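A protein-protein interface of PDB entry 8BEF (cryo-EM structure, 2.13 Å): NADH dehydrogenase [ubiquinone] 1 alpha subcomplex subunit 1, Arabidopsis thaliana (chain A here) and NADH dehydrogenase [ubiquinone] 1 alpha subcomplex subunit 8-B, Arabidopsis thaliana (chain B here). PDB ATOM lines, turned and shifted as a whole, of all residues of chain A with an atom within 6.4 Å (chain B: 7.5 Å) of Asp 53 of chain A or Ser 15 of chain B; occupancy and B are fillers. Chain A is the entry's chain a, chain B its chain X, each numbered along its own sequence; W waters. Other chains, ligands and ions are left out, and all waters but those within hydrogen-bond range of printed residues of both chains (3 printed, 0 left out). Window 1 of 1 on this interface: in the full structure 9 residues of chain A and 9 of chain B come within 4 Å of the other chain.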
ATOM      1  N   ARG A  36      -9.429  -0.403 -27.703  1.00  0.00           N
ATOM      2  CA  ARG A  36      -8.250  -1.241 -27.587  1.00  0.00           C
ATOM      3  C   ARG A  36      -7.600  -1.331 -28.959  1.00  0.00           C
ATOM      4  O   ARG A  36      -8.261  -1.105 -29.977  1.00  0.00           O
ATOM      5  CB  ARG A  36      -8.597  -2.644 -27.068  1.00  0.00           C
ATOM      6  CG  ARG A  36      -9.829  -3.268 -27.697  1.00  0.00           C
ATOM      7  CD  ARG A  36     -10.162  -4.567 -26.993  1.00  0.00           C
ATOM      8  NE  ARG A  36     -11.331  -5.237 -27.545  1.00  0.00           N
ATOM      9  CZ  ARG A  36     -11.735  -6.447 -27.182  1.00  0.00           C
ATOM     10  NH1 ARG A  36     -11.073  -7.156 -26.283  1.00  0.00           N
ATOM     11  NH2 ARG A  36     -12.828  -6.958 -27.738  1.00  0.00           N
ATOM     12  N   ALA A  48     -17.335 -14.220 -32.657  1.00  0.00           N
ATOM     13  CA  ALA A  48     -18.397 -14.772 -31.820  1.00  0.00           C
ATOM     14  C   ALA A  48     -18.235 -14.343 -30.366  1.00  0.00           C
ATOM     15  O   ALA A  48     -19.225 -14.056 -29.682  1.00  0.00           O
ATOM     16  CB  ALA A  48     -18.421 -16.297 -31.934  1.00  0.00           C
ATOM     17  N   MET A  49     -16.993 -14.289 -29.879  1.00  0.00           N
ATOM     18  CA  MET A  49     -16.735 -13.823 -28.520  1.00  0.00           C
ATOM     19  C   MET A  49     -17.189 -12.384 -28.328  1.00  0.00           C
ATOM     20  O   MET A  49     -17.832 -12.059 -27.329  1.00  0.00           O
ATOM     21  CB  MET A  49     -15.248 -13.965 -28.186  1.00  0.00           C
ATOM     22  CG  MET A  49     -14.702 -15.372 -27.863  1.00  0.00           C
ATOM     23  SD  MET A  49     -15.689 -16.540 -26.883  1.00  0.00           S
ATOM     24  CE  MET A  49     -16.943 -17.110 -28.025  1.00  0.00           C
ATOM     25  N   GLU A  50     -16.855 -11.503 -29.273  1.00  0.00           N
ATOM     26  CA  GLU A  50     -17.269 -10.107 -29.156  1.00  0.00           C
ATOM     27  C   GLU A  50     -18.787  -9.959 -29.215  1.00  0.00           C
ATOM     28  O   GLU A  50     -19.377  -9.204 -28.427  1.00  0.00           O
ATOM     29  CB  GLU A  50     -16.590  -9.267 -30.240  1.00  0.00           C
ATOM     30  CG  GLU A  50     -15.080  -9.150 -30.069  1.00  0.00           C
ATOM     31  CD  GLU A  50     -14.400  -8.378 -31.184  1.00  0.00           C
ATOM     32  OE1 GLU A  50     -15.075  -8.089 -32.198  1.00  0.00           O
ATOM     33  OE2 GLU A  50     -13.192  -8.088 -31.070  1.00  0.00           O
ATOM     34  N   ARG A  51     -19.442 -10.683 -30.128  1.00  0.00           N
ATOM     35  CA  ARG A  51     -20.896 -10.587 -30.219  1.00  0.00           C
ATOM     36  C   ARG A  51     -21.569 -11.092 -28.945  1.00  0.00           C
ATOM     37  O   ARG A  51     -22.526 -10.479 -28.462  1.00  0.00           O
ATOM     38  CB  ARG A  51     -21.412 -11.351 -31.440  1.00  0.00           C
ATOM     39  CG  ARG A  51     -21.293 -10.576 -32.742  1.00  0.00           C
ATOM     40  CD  ARG A  51     -21.055 -11.504 -33.917  1.00  0.00           C
ATOM     41  NE  ARG A  51     -20.605 -10.789 -35.104  1.00  0.00           N
ATOM     42  CZ  ARG A  51     -20.874 -11.162 -36.349  1.00  0.00           C
ATOM     43  NH1 ARG A  51     -21.617 -12.224 -36.607  1.00  0.00           N
ATOM     44  NH2 ARG A  51     -20.377 -10.454 -37.357  1.00  0.00           N
ATOM     45  N   ARG A  52     -21.087 -12.204 -28.384  1.00  0.00           N
ATOM     46  CA  ARG A  52     -21.670 -12.705 -27.143  1.00  0.00           C
ATOM     47  C   ARG A  52     -21.330 -11.804 -25.958  1.00  0.00           C
ATOM     48  O   ARG A  52     -22.143 -11.656 -25.035  1.00  0.00           O
ATOM     49  CB  ARG A  52     -21.201 -14.140 -26.904  1.00  0.00           C
ATOM     50  CG  ARG A  52     -21.581 -14.727 -25.567  1.00  0.00           C
ATOM     51  CD  ARG A  52     -20.414 -15.477 -24.965  1.00  0.00           C
ATOM     52  NE  ARG A  52     -20.643 -15.847 -23.575  1.00  0.00           N
ATOM     53  CZ  ARG A  52     -19.944 -15.373 -22.553  1.00  0.00           C
ATOM     54  NH1 ARG A  52     -18.975 -14.491 -22.729  1.00  0.00           N
ATOM     55  NH2 ARG A  52     -20.226 -15.793 -21.324  1.00  0.00           N
ATOM     56  N   ASP A  53     -20.154 -11.172 -25.982  1.00  0.00           N
ATOM     57  CA  ASP A  53     -19.749 -10.298 -24.889  1.00  0.00           C
ATOM     58  C   ASP A  53     -20.572  -9.025 -24.862  1.00  0.00           C
ATOM     59  O   ASP A  53     -20.797  -8.465 -23.785  1.00  0.00           O
ATOM     60  CB  ASP A  53     -18.262  -9.961 -25.003  1.00  0.00           C
ATOM     61  CG  ASP A  53     -17.400 -10.844 -24.128  1.00  0.00           C
ATOM     62  OD1 ASP A  53     -17.857 -11.949 -23.773  1.00  0.00           O
ATOM     63  OD2 ASP A  53     -16.266 -10.440 -23.799  1.00  0.00           O
ATOM     64  N   LYS A  54     -21.021  -8.548 -26.028  1.00  0.00           N
ATOM     65  CA  LYS A  54     -21.947  -7.421 -26.037  1.00  0.00           C
ATOM     66  C   LYS A  54     -23.162  -7.716 -25.165  1.00  0.00           C
ATOM     67  O   LYS A  54     -23.556  -6.897 -24.329  1.00  0.00           O
ATOM     68  CB  LYS A  54     -22.394  -7.091 -27.464  1.00  0.00           C
ATOM     69  CG  LYS A  54     -21.290  -6.682 -28.416  1.00  0.00           C
ATOM     70  CD  LYS A  54     -21.831  -6.566 -29.831  1.00  0.00           C
ATOM     71  CE  LYS A  54     -20.719  -6.393 -30.848  1.00  0.00           C
ATOM     72  NZ  LYS A  54     -21.250  -6.374 -32.240  1.00  0.00           N
ATOM     73  N   LYS A  55     -23.760  -8.897 -25.342  1.00  0.00           N
ATOM     74  CA  LYS A  55     -24.891  -9.294 -24.509  1.00  0.00           C
ATOM     75  C   LYS A  55     -24.478  -9.428 -23.048  1.00  0.00           C
ATOM     76  O   LYS A  55     -25.089  -8.821 -22.161  1.00  0.00           O
ATOM     77  CB  LYS A  55     -25.488 -10.605 -25.018  1.00  0.00           C
ATOM     78  CG  LYS A  55     -25.740 -10.659 -26.518  1.00  0.00           C
ATOM     79  CD  LYS A  55     -26.462  -9.421 -27.019  1.00  0.00           C
ATOM     80  CE  LYS A  55     -26.513  -9.394 -28.540  1.00  0.00           C
ATOM     81  NZ  LYS A  55     -27.685  -8.625 -29.043  1.00  0.00           N
ATOM     82  N   VAL A  56     -23.417 -10.197 -22.782  1.00  0.00           N
ATOM     83  CA  VAL A  56     -23.016 -10.466 -21.402  1.00  0.00           C
ATOM     84  C   VAL A  56     -22.670  -9.186 -20.643  1.00  0.00           C
ATOM     85  O   VAL A  56     -22.775  -9.149 -19.412  1.00  0.00           O
ATOM     86  CB  VAL A  56     -21.845 -11.474 -21.376  1.00  0.00           C
ATOM     87  CG1 VAL A  56     -21.482 -11.850 -19.953  1.00  0.00           C
ATOM     88  CG2 VAL A  56     -22.218 -12.730 -22.142  1.00  0.00           C
ATOM     89  N   VAL A  57     -22.293  -8.120 -21.345  1.00  0.00           N
ATOM     90  CA  VAL A  57     -22.007  -6.849 -20.690  1.00  0.00           C
ATOM     91  C   VAL A  57     -23.278  -6.017 -20.577  1.00  0.00           C
ATOM     92  O   VAL A  57     -23.689  -5.648 -19.471  1.00  0.00           O
ATOM     93  CB  VAL A  57     -20.908  -6.073 -21.439  1.00  0.00           C
ATOM     94  CG1 VAL A  57     -20.804  -4.651 -20.908  1.00  0.00           C
ATOM     95  CG2 VAL A  57     -19.575  -6.791 -21.307  1.00  0.00           C
ATOM     96  N   GLU A  58     -23.909  -5.714 -21.717  1.00  0.00           N
ATOM     97  CA  GLU A  58     -25.016  -4.762 -21.730  1.00  0.00           C
ATOM     98  C   GLU A  58     -26.204  -5.267 -20.920  1.00  0.00           C
ATOM     99  O   GLU A  58     -26.899  -4.479 -20.267  1.00  0.00           O
ATOM    100  CB  GLU A  58     -25.429  -4.467 -23.173  1.00  0.00           C
ATOM    101  CG  GLU A  58     -26.537  -3.438 -23.315  1.00  0.00           C
ATOM    102  CD  GLU A  58     -26.812  -3.076 -24.762  1.00  0.00           C
ATOM    103  OE1 GLU A  58     -26.546  -3.917 -25.646  1.00  0.00           O
ATOM    104  OE2 GLU A  58     -27.293  -1.952 -25.015  1.00  0.00           O
ATOM    105  N   ILE B  12     -18.074 -10.604 -14.131  1.00  0.00           N
ATOM    106  CA  ILE B  12     -18.830 -10.816 -15.361  1.00  0.00           C
ATOM    107  C   ILE B  12     -18.040 -11.810 -16.203  1.00  0.00           C
ATOM    108  O   ILE B  12     -16.877 -11.544 -16.542  1.00  0.00           O
ATOM    109  CB  ILE B  12     -19.073  -9.499 -16.111  1.00  0.00           C
ATOM    110  CG1 ILE B  12     -19.591  -8.427 -15.150  1.00  0.00           C
ATOM    111  CG2 ILE B  12     -20.050  -9.707 -17.257  1.00  0.00           C
ATOM    112  CD1 ILE B  12     -20.966  -8.721 -14.592  1.00  0.00           C
ATOM    113  N   PRO B  13     -18.618 -12.955 -16.558  1.00  0.00           N
ATOM    114  CA  PRO B  13     -17.868 -13.990 -17.289  1.00  0.00           C
ATOM    115  C   PRO B  13     -17.698 -13.648 -18.765  1.00  0.00           C
ATOM    116  O   PRO B  13     -18.178 -14.348 -19.659  1.00  0.00           O
ATOM    117  CB  PRO B  13     -18.736 -15.233 -17.065  1.00  0.00           C
ATOM    118  CG  PRO B  13     -20.118 -14.690 -17.008  1.00  0.00           C
ATOM    119  CD  PRO B  13     -20.024 -13.341 -16.347  1.00  0.00           C
ATOM    120  N   THR B  14     -16.999 -12.548 -19.024  1.00  0.00           N
ATOM    121  CA  THR B  14     -16.722 -12.123 -20.384  1.00  0.00           C
ATOM    122  C   THR B  14     -15.681 -13.041 -21.019  1.00  0.00           C
ATOM    123  O   THR B  14     -15.124 -13.937 -20.380  1.00  0.00           O
ATOM    124  CB  THR B  14     -16.239 -10.676 -20.402  1.00  0.00           C
ATOM    125  OG1 THR B  14     -15.041 -10.567 -19.625  1.00  0.00           O
ATOM    126  CG2 THR B  14     -17.299  -9.765 -19.821  1.00  0.00           C
ATOM    127  N   SER B  15     -15.410 -12.799 -22.302  1.00  0.00           N
ATOM    128  CA  SER B  15     -14.403 -13.586 -23.005  1.00  0.00           C
ATOM    129  C   SER B  15     -13.031 -13.419 -22.368  1.00  0.00           C
ATOM    130  O   SER B  15     -12.256 -14.377 -22.289  1.00  0.00           O
ATOM    131  CB  SER B  15     -14.371 -13.192 -24.484  1.00  0.00           C
ATOM    132  OG  SER B  15     -13.966 -11.846 -24.654  1.00  0.00           O
ATOM    133  N   ALA B  16     -12.710 -12.206 -21.911  1.00  0.00           N
ATOM    134  CA  ALA B  16     -11.414 -11.974 -21.281  1.00  0.00           C
ATOM    135  C   ALA B  16     -11.266 -12.787 -20.000  1.00  0.00           C
ATOM    136  O   ALA B  16     -10.243 -13.444 -19.785  1.00  0.00           O
ATOM    137  CB  ALA B  16     -11.226 -10.482 -20.998  1.00  0.00           C
ATOM    138  N   VAL B  17     -12.286 -12.760 -19.138  1.00  0.00           N
ATOM    139  CA  VAL B  17     -12.208 -13.481 -17.867  1.00  0.00           C
ATOM    140  C   VAL B  17     -12.065 -14.978 -18.113  1.00  0.00           C
ATOM    141  O   VAL B  17     -11.195 -15.644 -17.535  1.00  0.00           O
ATOM    142  CB  VAL B  17     -13.441 -13.169 -16.999  1.00  0.00           C
ATOM    143  CG1 VAL B  17     -13.510 -14.121 -15.818  1.00  0.00           C
ATOM    144  CG2 VAL B  17     -13.406 -11.719 -16.531  1.00  0.00           C
ATOM    145  N   LEU B  18     -12.903 -15.524 -18.996  1.00  0.00           N
ATOM    146  CA  LEU B  18     -12.868 -16.956 -19.269  1.00  0.00           C
ATOM    147  C   LEU B  18     -11.545 -17.368 -19.903  1.00  0.00           C
ATOM    148  O   LEU B  18     -10.952 -18.378 -19.516  1.00  0.00           O
ATOM    149  CB  LEU B  18     -14.045 -17.346 -20.162  1.00  0.00           C
ATOM    150  CG  LEU B  18     -15.421 -17.137 -19.528  1.00  0.00           C
ATOM    151  CD1 LEU B  18     -16.530 -17.315 -20.551  1.00  0.00           C
ATOM    152  CD2 LEU B  18     -15.608 -18.081 -18.353  1.00  0.00           C
ATOM    153  N   THR B  19     -11.065 -16.597 -20.881  1.00  0.00           N
ATOM    154  CA  THR B  19      -9.805 -16.945 -21.527  1.00  0.00           C
ATOM    155  C   THR B  19      -8.646 -16.879 -20.542  1.00  0.00           C
ATOM    156  O   THR B  19      -7.794 -17.773 -20.519  1.00  0.00           O
ATOM    157  CB  THR B  19      -9.548 -16.038 -22.733  1.00  0.00           C
ATOM    158  OG1 THR B  19     -10.736 -15.950 -23.528  1.00  0.00           O
ATOM    159  CG2 THR B  19      -8.431 -16.610 -23.588  1.00  0.00           C
ATOM    160  N   ALA B  20      -8.611 -15.843 -19.700  1.00  0.00           N
ATOM    161  CA  ALA B  20      -7.550 -15.743 -18.706  1.00  0.00           C
ATOM    162  C   ALA B  20      -7.608 -16.889 -17.701  1.00  0.00           C
ATOM    163  O   ALA B  20      -6.562 -17.347 -17.228  1.00  0.00           O
ATOM    164  CB  ALA B  20      -7.626 -14.397 -17.985  1.00  0.00           C
ATOM    165  N   SER B  21      -8.806 -17.367 -17.370  1.00  0.00           N
ATOM    166  CA  SER B  21      -8.959 -18.445 -16.400  1.00  0.00           C
ATOM    167  C   SER B  21      -9.009 -19.831 -17.035  1.00  0.00           C
ATOM    168  O   SER B  21      -9.223 -20.808 -16.313  1.00  0.00           O
ATOM    169  CB  SER B  21     -10.227 -18.226 -15.570  1.00  0.00           C
ATOM    170  OG  SER B  21     -10.160 -17.013 -14.847  1.00  0.00           O
ATOM    171  N   VAL B  79      -6.767 -10.089 -16.370  1.00  0.00           N
ATOM    172  CA  VAL B  79      -7.980  -9.946 -17.169  1.00  0.00           C
ATOM    173  C   VAL B  79      -7.942  -8.650 -17.968  1.00  0.00           C
ATOM    174  O   VAL B  79      -8.336  -8.616 -19.139  1.00  0.00           O
ATOM    175  CB  VAL B  79      -9.221 -10.026 -16.258  1.00  0.00           C
ATOM    176  CG1 VAL B  79     -10.456  -9.513 -16.976  1.00  0.00           C
ATOM    177  CG2 VAL B  79      -9.432 -11.453 -15.774  1.00  0.00           C
ATOM    178  N   MET B  82      -5.499  -9.053 -20.845  1.00  0.00           N
ATOM    179  CA  MET B  82      -6.071  -9.972 -21.822  1.00  0.00           C
ATOM    180  C   MET B  82      -7.157  -9.296 -22.648  1.00  0.00           C
ATOM    181  O   MET B  82      -7.256  -9.519 -23.860  1.00  0.00           O
ATOM    182  CB  MET B  82      -6.628 -11.204 -21.111  1.00  0.00           C
ATOM    183  CG  MET B  82      -5.572 -12.222 -20.733  1.00  0.00           C
ATOM    184  SD  MET B  82      -4.860 -13.027 -22.177  1.00  0.00           S
ATOM    185  CE  MET B  82      -5.941 -14.442 -22.302  1.00  0.00           C
ATOM    186  N   TYR B  83      -7.993  -8.477 -22.008  1.00  0.00           N
ATOM    187  CA  TYR B  83      -8.999  -7.738 -22.761  1.00  0.00           C
ATOM    188  C   TYR B  83      -8.347  -6.700 -23.665  1.00  0.00           C
ATOM    189  O   TYR B  83      -8.789  -6.490 -24.799  1.00  0.00           O
ATOM    190  CB  TYR B  83      -9.999  -7.073 -21.813  1.00  0.00           C
ATOM    191  CG  TYR B  83     -10.832  -6.012 -22.492  1.00  0.00           C
ATOM    192  CD1 TYR B  83     -12.012  -6.347 -23.140  1.00  0.00           C
ATOM    193  CD2 TYR B  83     -10.437  -4.677 -22.495  1.00  0.00           C
ATOM    194  CE1 TYR B  83     -12.773  -5.391 -23.776  1.00  0.00           C
ATOM    195  CE2 TYR B  83     -11.190  -3.716 -23.128  1.00  0.00           C
ATOM    196  CZ  TYR B  83     -12.358  -4.077 -23.767  1.00  0.00           C
ATOM    197  OH  TYR B  83     -13.114  -3.119 -24.395  1.00  0.00           O
ATOM    198  N   THR B  86      -6.982  -8.456 -26.663  1.00  0.00           N
ATOM    199  CA  THR B  86      -7.934  -9.416 -27.223  1.00  0.00           C
ATOM    200  C   THR B  86      -7.439 -10.852 -27.031  1.00  0.00           C
ATOM    201  O   THR B  86      -7.292 -11.626 -27.981  1.00  0.00           O
ATOM    202  CB  THR B  86      -8.223  -9.112 -28.697  1.00  0.00           C
ATOM    203  OG1 THR B  86      -8.438  -7.707 -28.858  1.00  0.00           O
ATOM    204  CG2 THR B  86      -9.482  -9.840 -29.162  1.00  0.00           C
ATOM    205  N   ASN B  87      -7.143 -11.187 -25.776  1.00  0.00           N
ATOM    206  CA  ASN B  87      -6.867 -12.558 -25.345  1.00  0.00           C
ATOM    207  C   ASN B  87      -5.632 -13.159 -26.015  1.00  0.00           C
ATOM    208  O   ASN B  87      -5.566 -14.368 -26.235  1.00  0.00           O
ATOM    209  CB  ASN B  87      -8.086 -13.458 -25.573  1.00  0.00           C
ATOM    210  CG  ASN B  87      -9.330 -12.925 -24.899  1.00  0.00           C
ATOM    211  OD1 ASN B  87      -9.281 -12.470 -23.758  1.00  0.00           O
ATOM    212  ND2 ASN B  87     -10.452 -12.968 -25.603  1.00  0.00           N
HETATM  213  O   HOH W   1     -14.639  -9.983 -27.475  1.00  0.00           O
HETATM  214  O   HOH W   2     -11.305  -9.624 -24.649  1.00  0.00           O
HETATM  215  O   HOH W   3     -13.838  -9.827 -22.771  1.00  0.00           O
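Arg 36 of chain A touches Thr 86 of chain B.
Ser 15 of chain B touches Met 49 of chain A.
NH1 of Arg 52 of chain A touches C of Thr 14 of chain B (3.98 Å).
Ser 15 of chain B touches Arg 52 of chain A (N to NH1, 3.97 Å).
Asp 53 of chain A touches Thr 14 of chain B.
Val 56 of chain A touches Ile 12 of chain B (O to CG2, 3.5 Å).
The backbone carbonyl oxygen (O) of Tyr 83 of chain B is in hydrogen-bond range of the guanidinium group (NH1) of Arg 36 of chain A (2.8 Å).
The guanidinium group (NH2) of Arg 52 of chain A sits at hydrogen-bond distance from the backbone carbonyl oxygen (O) of Pro 13 of chain B (3.0 Å).
The side-chain carboxylate (OD2) of Asp 53 of chain A sits at hydrogen-bond distance from the side-chain hydroxyl (OG) of Ser 15 of chain B (2.8 Å).
NH2 of Arg 36 of chain A lies within salt-bridge range of OE2 of Glu 50 of chain A (3.5 Å).
OD1 of Asp 53 of chain A lies within salt-bridge range of NH1 of Arg 52 of chain A.
The side-chain hydroxyl of Thr 19 of chain B is in hydrogen-bond range of the backbone carbonyl oxygen of Ser 15 of chain B (2.5 Å).
Of the printed residues of chain B, Arg 36 of chain A touches Tyr 83 and Thr 86.
Of the printed residues of chain B, Met 49 of chain A touches Ser 15.
Asp 53 of chain A touches two residues of chain B.
Lys 55 of chain A touches none of the printed residues of chain B.
Of the printed residues of chain A, Pro 13 of chain B touches Arg 52.
Of chain A, only Met 49 (3.9 Å), Arg 52 (3.97 Å) and Asp 53 (2.8 Å) come within 4 Å of Ser 15 of chain B.
Asn 87 of chain B touches none of the printed residues of chain A.
The nearest residue of chain B that does not touch Asp 53 of chain A is Ala 16 of chain B (4.4 Å).
Water W3 lies within hydrogen-bond range of OD2 of Asp 53 of chain A (2.7 Å), OG of Ser 15 of chain B (2.8 Å), N of Ala 16 of chain B (2.8 Å) and OG1 of Thr 14 of chain B (3.4 Å).
Water W2 lies within hydrogen-bond range of NH1 of Arg 36 of chain A (3.0 Å) and OG of Ser 15 of chain B (3.5 Å).
Water W1 bridges the backbone NH (N) of Glu 50 of chain A and the side-chain hydroxyl (OG) of Ser 15 of chain B.
Of the 12 printed residues of chain A, 5 touch a printed residue of chain B.
Hydrophobic or aromatic side chains of chain A within 4 Å of the printed part of chain B: Met 49 and Val 56.
Along chain A the printed residues that touch a printed residue of chain B span positions 36 to 56.
Of the 15 printed residues of chain B, 6 touch a printed residue of chain A.
Hydrophobic or aromatic side chains of chain B that line the printed part of chain A: Ile 12 and Tyr 83.
Along chain B the printed residues that touch a printed residue of chain A span positions 12 to 86.
Among the printed residues, 9 pairs touch across the chains.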
